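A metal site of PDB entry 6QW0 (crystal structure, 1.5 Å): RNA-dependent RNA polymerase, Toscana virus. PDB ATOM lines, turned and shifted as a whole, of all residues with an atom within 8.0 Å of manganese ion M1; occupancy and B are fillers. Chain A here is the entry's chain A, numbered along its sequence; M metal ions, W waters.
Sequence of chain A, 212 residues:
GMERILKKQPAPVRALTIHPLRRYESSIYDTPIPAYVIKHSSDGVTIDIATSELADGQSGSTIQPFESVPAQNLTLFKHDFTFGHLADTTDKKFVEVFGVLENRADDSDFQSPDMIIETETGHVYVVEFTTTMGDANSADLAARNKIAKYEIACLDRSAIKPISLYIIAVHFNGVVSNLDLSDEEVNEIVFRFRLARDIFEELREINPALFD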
ATOM      1  N   LEU A  76     -36.512 -16.753   6.711  1.00  0.00           N
ATOM      2  CA  LEU A  76     -35.994 -17.864   5.933  1.00  0.00           C
ATOM      3  C   LEU A  76     -36.923 -19.079   5.973  1.00  0.00           C
ATOM      4  O   LEU A  76     -36.501 -20.192   5.633  1.00  0.00           O
ATOM      5  CB  LEU A  76     -34.595 -18.253   6.425  1.00  0.00           C
ATOM      6  CG  LEU A  76     -33.490 -17.306   5.941  1.00  0.00           C
ATOM      7  CD1 LEU A  76     -32.160 -17.654   6.570  1.00  0.00           C
ATOM      8  CD2 LEU A  76     -33.401 -17.321   4.414  1.00  0.00           C
ATOM      9  N   HIS A  79     -37.501 -20.965   2.539  1.00  0.00           N
ATOM     10  CA  HIS A  79     -36.313 -21.708   2.120  1.00  0.00           C
ATOM     11  C   HIS A  79     -36.118 -22.953   2.985  1.00  0.00           C
ATOM     12  O   HIS A  79     -35.946 -24.071   2.462  1.00  0.00           O
ATOM     13  CB  HIS A  79     -35.104 -20.768   2.199  1.00  0.00           C
ATOM     14  CG  HIS A  79     -33.767 -21.423   2.016  1.00  0.00           C
ATOM     15  ND1 HIS A  79     -33.138 -22.134   3.015  1.00  0.00           N
ATOM     16  CD2 HIS A  79     -32.904 -21.390   0.968  1.00  0.00           C
ATOM     17  CE1 HIS A  79     -31.959 -22.542   2.581  1.00  0.00           C
ATOM     18  NE2 HIS A  79     -31.795 -22.110   1.352  1.00  0.00           N
ATOM     19  N   ASP A  80     -36.169 -22.783   4.306  1.00  0.00           N
ATOM     20  CA  ASP A  80     -35.858 -23.881   5.202  1.00  0.00           C
ATOM     21  C   ASP A  80     -36.922 -24.965   5.145  1.00  0.00           C
ATOM     22  O   ASP A  80     -36.598 -26.157   5.169  1.00  0.00           O
ATOM     23  CB  ASP A  80     -35.694 -23.348   6.630  1.00  0.00           C
ATOM     24  CG  ASP A  80     -34.405 -22.573   6.797  1.00  0.00           C
ATOM     25  OD1 ASP A  80     -33.591 -22.554   5.847  1.00  0.00           O
ATOM     26  OD2 ASP A  80     -34.204 -21.978   7.874  1.00  0.00           O
ATOM     27  N   PHE A  83     -36.736 -27.261   1.739  1.00  0.00           N
ATOM     28  CA  PHE A  83     -35.647 -28.211   1.609  1.00  0.00           C
ATOM     29  C   PHE A  83     -35.430 -29.025   2.878  1.00  0.00           C
ATOM     30  O   PHE A  83     -34.432 -29.761   2.970  1.00  0.00           O
ATOM     31  CB  PHE A  83     -34.372 -27.475   1.175  1.00  0.00           C
ATOM     32  CG  PHE A  83     -34.508 -26.799  -0.157  1.00  0.00           C
ATOM     33  CD1 PHE A  83     -34.383 -27.521  -1.328  1.00  0.00           C
ATOM     34  CD2 PHE A  83     -34.782 -25.441  -0.243  1.00  0.00           C
ATOM     35  CE1 PHE A  83     -34.524 -26.915  -2.577  1.00  0.00           C
ATOM     36  CE2 PHE A  83     -34.919 -24.811  -1.496  1.00  0.00           C
ATOM     37  CZ  PHE A  83     -34.778 -25.560  -2.655  1.00  0.00           C
ATOM     38  N   SER A 112     -21.060 -20.174   4.359  1.00  0.00           N
ATOM     39  CA  SER A 112     -21.788 -21.340   4.874  1.00  0.00           C
ATOM     40  C   SER A 112     -22.848 -21.789   3.877  1.00  0.00           C
ATOM     41  O   SER A 112     -24.024 -21.433   3.995  1.00  0.00           O
ATOM     42  CB  SER A 112     -22.418 -21.031   6.234  1.00  0.00           C
ATOM     43  OG  SER A 112     -23.088 -22.161   6.751  1.00  0.00           O
ATOM     44  N   PRO A 113     -22.470 -22.592   2.881  1.00  0.00           N
ATOM     45  CA  PRO A 113     -23.466 -23.180   1.982  1.00  0.00           C
ATOM     46  C   PRO A 113     -24.395 -24.104   2.744  1.00  0.00           C
ATOM     47  O   PRO A 113     -24.146 -24.485   3.893  1.00  0.00           O
ATOM     48  CB  PRO A 113     -22.631 -23.958   0.954  1.00  0.00           C
ATOM     49  CG  PRO A 113     -21.174 -23.672   1.296  1.00  0.00           C
ATOM     50  CD  PRO A 113     -21.146 -23.209   2.713  1.00  0.00           C
ATOM     51  N   ASP A 114     -25.499 -24.487   2.102  1.00  0.00           N
ATOM     52  CA  ASP A 114     -26.512 -25.282   2.811  1.00  0.00           C
ATOM     53  C   ASP A 114     -25.985 -26.650   3.236  1.00  0.00           C
ATOM     54  O   ASP A 114     -26.403 -27.176   4.270  1.00  0.00           O
ATOM     55  CB  ASP A 114     -27.758 -25.456   1.940  1.00  0.00           C
ATOM     56  CG  ASP A 114     -28.624 -24.207   1.928  1.00  0.00           C
ATOM     57  OD1 ASP A 114     -28.996 -23.721   3.020  1.00  0.00           O
ATOM     58  OD2 ASP A 114     -28.916 -23.684   0.837  1.00  0.00           O
ATOM     59  N   MET A 115     -25.106 -27.253   2.439  1.00  0.00           N
ATOM     60  CA  MET A 115     -24.513 -28.536   2.813  1.00  0.00           C
ATOM     61  C   MET A 115     -23.049 -28.580   2.382  1.00  0.00           C
ATOM     62  O   MET A 115     -22.709 -28.130   1.283  1.00  0.00           O
ATOM     63  CB  MET A 115     -25.264 -29.715   2.178  1.00  0.00           C
ATOM     64  CG  MET A 115     -26.807 -29.704   2.272  1.00  0.00           C
ATOM     65  SD  MET A 115     -27.555 -31.324   1.524  1.00  0.00           S
ATOM     66  CE  MET A 115     -27.067 -32.519   3.006  1.00  0.00           C
ATOM     67  N   VAL A 127     -23.498 -28.198  -1.537  1.00  0.00           N
ATOM     68  CA  VAL A 127     -24.858 -28.129  -2.054  1.00  0.00           C
ATOM     69  C   VAL A 127     -25.502 -26.834  -1.560  1.00  0.00           C
ATOM     70  O   VAL A 127     -25.431 -26.518  -0.372  1.00  0.00           O
ATOM     71  CB  VAL A 127     -25.705 -29.343  -1.638  1.00  0.00           C
ATOM     72  CG1 VAL A 127     -27.070 -29.281  -2.317  1.00  0.00           C
ATOM     73  CG2 VAL A 127     -25.011 -30.654  -1.990  1.00  0.00           C
ATOM     74  N   GLU A 128     -26.110 -26.084  -2.472  1.00  0.00           N
ATOM     75  CA  GLU A 128     -26.780 -24.840  -2.091  1.00  0.00           C
ATOM     76  C   GLU A 128     -28.211 -24.867  -2.607  1.00  0.00           C
ATOM     77  O   GLU A 128     -28.438 -25.219  -3.773  1.00  0.00           O
ATOM     78  CB  GLU A 128     -26.043 -23.604  -2.609  1.00  0.00           C
ATOM     79  CG  GLU A 128     -26.745 -22.306  -2.297  1.00  0.00           C
ATOM     80  CD  GLU A 128     -26.844 -22.000  -0.796  1.00  0.00           C
ATOM     81  OE1 GLU A 128     -26.087 -22.551   0.028  1.00  0.00           O
ATOM     82  OE2 GLU A 128     -27.710 -21.189  -0.439  1.00  0.00           O
ATOM     83  N   PHE A 129     -29.148 -24.511  -1.737  1.00  0.00           N
ATOM     84  CA  PHE A 129     -30.569 -24.432  -2.044  1.00  0.00           C
ATOM     85  C   PHE A 129     -30.989 -22.982  -2.243  1.00  0.00           C
ATOM     86  O   PHE A 129     -30.473 -22.081  -1.591  1.00  0.00           O
ATOM     87  CB  PHE A 129     -31.440 -25.007  -0.903  1.00  0.00           C
ATOM     88  CG  PHE A 129     -31.006 -26.354  -0.370  1.00  0.00           C
ATOM     89  CD1 PHE A 129     -30.699 -27.413  -1.200  1.00  0.00           C
ATOM     90  CD2 PHE A 129     -31.004 -26.555   1.002  1.00  0.00           C
ATOM     91  CE1 PHE A 129     -30.329 -28.646  -0.658  1.00  0.00           C
ATOM     92  CE2 PHE A 129     -30.634 -27.789   1.544  1.00  0.00           C
ATOM     93  CZ  PHE A 129     -30.298 -28.824   0.710  1.00  0.00           C
ATOM     94  N   THR A 130     -31.953 -22.759  -3.128  1.00  0.00           N
ATOM     95  CA  THR A 130     -32.460 -21.403  -3.276  1.00  0.00           C
ATOM     96  C   THR A 130     -33.875 -21.487  -3.843  1.00  0.00           C
ATOM     97  O   THR A 130     -34.306 -22.543  -4.313  1.00  0.00           O
ATOM     98  CB  THR A 130     -31.524 -20.537  -4.138  1.00  0.00           C
ATOM     99  OG1 THR A 130     -31.895 -19.151  -4.071  1.00  0.00           O
ATOM    100  CG2 THR A 130     -31.528 -21.000  -5.577  1.00  0.00           C
ATOM    101  N   THR A 131     -34.611 -20.383  -3.718  1.00  0.00           N
ATOM    102  CA  THR A 131     -36.000 -20.307  -4.168  1.00  0.00           C
ATOM    103  C   THR A 131     -36.171 -19.073  -5.046  1.00  0.00           C
ATOM    104  O   THR A 131     -35.322 -18.178  -5.053  1.00  0.00           O
ATOM    105  CB  THR A 131     -36.984 -20.211  -2.998  1.00  0.00           C
ATOM    106  OG1 THR A 131     -36.824 -18.941  -2.355  1.00  0.00           O
ATOM    107  CG2 THR A 131     -36.738 -21.320  -1.977  1.00  0.00           C
ATOM    108  N   LYS A 146     -26.160 -18.359  -7.173  1.00  0.00           N
ATOM    109  CA  LYS A 146     -25.544 -19.134  -6.083  1.00  0.00           C
ATOM    110  C   LYS A 146     -24.223 -19.742  -6.532  1.00  0.00           C
ATOM    111  O   LYS A 146     -23.295 -19.847  -5.715  1.00  0.00           O
ATOM    112  CB  LYS A 146     -26.487 -20.218  -5.590  1.00  0.00           C
ATOM    113  CG  LYS A 146     -27.713 -19.699  -4.871  1.00  0.00           C
ATOM    114  CD  LYS A 146     -27.346 -18.783  -3.721  1.00  0.00           C
ATOM    115  CE  LYS A 146     -28.590 -18.417  -2.899  1.00  0.00           C
ATOM    116  NZ  LYS A 146     -28.247 -17.478  -1.789  1.00  0.00           N
ATOM    117  N   LYS A 149     -21.822 -17.083  -6.096  1.00  0.00           N
ATOM    118  CA  LYS A 149     -21.570 -16.739  -4.707  1.00  0.00           C
ATOM    119  C   LYS A 149     -20.519 -17.646  -4.079  1.00  0.00           C
ATOM    120  O   LYS A 149     -19.741 -17.195  -3.233  1.00  0.00           O
ATOM    121  CB  LYS A 149     -22.891 -16.809  -3.923  1.00  0.00           C
ATOM    122  CG  LYS A 149     -22.761 -16.501  -2.440  1.00  0.00           C
ATOM    123  CD  LYS A 149     -24.092 -16.736  -1.733  1.00  0.00           C
ATOM    124  CE  LYS A 149     -24.051 -16.290  -0.281  1.00  0.00           C
ATOM    125  NZ  LYS A 149     -23.972 -14.796  -0.184  1.00  0.00           N
ATOM    126  N   TYR A 150     -20.479 -18.924  -4.486  1.00  0.00           N
ATOM    127  CA  TYR A 150     -19.624 -19.895  -3.829  1.00  0.00           C
ATOM    128  C   TYR A 150     -18.463 -20.406  -4.678  1.00  0.00           C
ATOM    129  O   TYR A 150     -17.623 -21.139  -4.151  1.00  0.00           O
ATOM    130  CB  TYR A 150     -20.475 -21.091  -3.376  1.00  0.00           C
ATOM    131  CG  TYR A 150     -21.415 -20.701  -2.264  1.00  0.00           C
ATOM    132  CD1 TYR A 150     -20.918 -20.332  -1.026  1.00  0.00           C
ATOM    133  CD2 TYR A 150     -22.791 -20.651  -2.455  1.00  0.00           C
ATOM    134  CE1 TYR A 150     -21.753 -19.948   0.010  1.00  0.00           C
ATOM    135  CE2 TYR A 150     -23.642 -20.273  -1.429  1.00  0.00           C
ATOM    136  CZ  TYR A 150     -23.117 -19.924  -0.205  1.00  0.00           C
ATOM    137  OH  TYR A 150     -23.931 -19.542   0.817  1.00  0.00           O
ATOM    138  N   ILE A 168     -29.750 -26.482  -6.114  1.00  0.00           N
ATOM    139  CA  ILE A 168     -31.178 -26.725  -6.365  1.00  0.00           C
ATOM    140  C   ILE A 168     -31.900 -25.385  -6.245  1.00  0.00           C
ATOM    141  O   ILE A 168     -31.924 -24.791  -5.159  1.00  0.00           O
ATOM    142  CB  ILE A 168     -31.797 -27.740  -5.392  1.00  0.00           C
ATOM    143  CG1 ILE A 168     -30.946 -29.010  -5.291  1.00  0.00           C
ATOM    144  CG2 ILE A 168     -33.210 -28.100  -5.844  1.00  0.00           C
ATOM    145  CD1 ILE A 168     -31.454 -30.001  -4.251  1.00  0.00           C
HETATM  146 MN    MN M   1     -29.703 -21.602   0.496  1.00  0.00          MN
HETATM  147 MN    MN M   2     -28.093 -21.246   4.053  1.00  0.00          MN
HETATM  148  O   HOH W   1     -29.191 -20.257   2.376  1.00  0.00           O
HETATM  149  O   HOH W   2     -30.198 -19.335   0.062  1.00  0.00           O
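OE2 of Glu 128 sits close to NZ of Lys 146. OD1 of Asp 80 sits at hydrogen-bond distance from ND1 of His 79 (2.9 Å). The backbone carbonyl oxygen of Glu 128 sits at hydrogen-bond distance from the backbone NH of Ile 168 (3.0 Å). The backbone carbonyl oxygen (O) of Val 127 sits at hydrogen-bond distance from the backbone NH (N) of Asp 114 (3.2 Å).
Manganese ion M1 is bound by the side-chain carboxylate (OE2) of Glu 128, the side-chain carboxylate (OD2) of Asp 114, the backbone carbonyl oxygen (O) of Phe 129, a ring nitrogen (NE2) of His 79, water W2 and water W1.
Four residues have an atom within 4 Å of manganese ion M1: His 79, Asp 114, Glu 128 and Phe 129. The nearest printed residue that does not touch manganese ion M1 is Thr 130 (4.4 Å).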
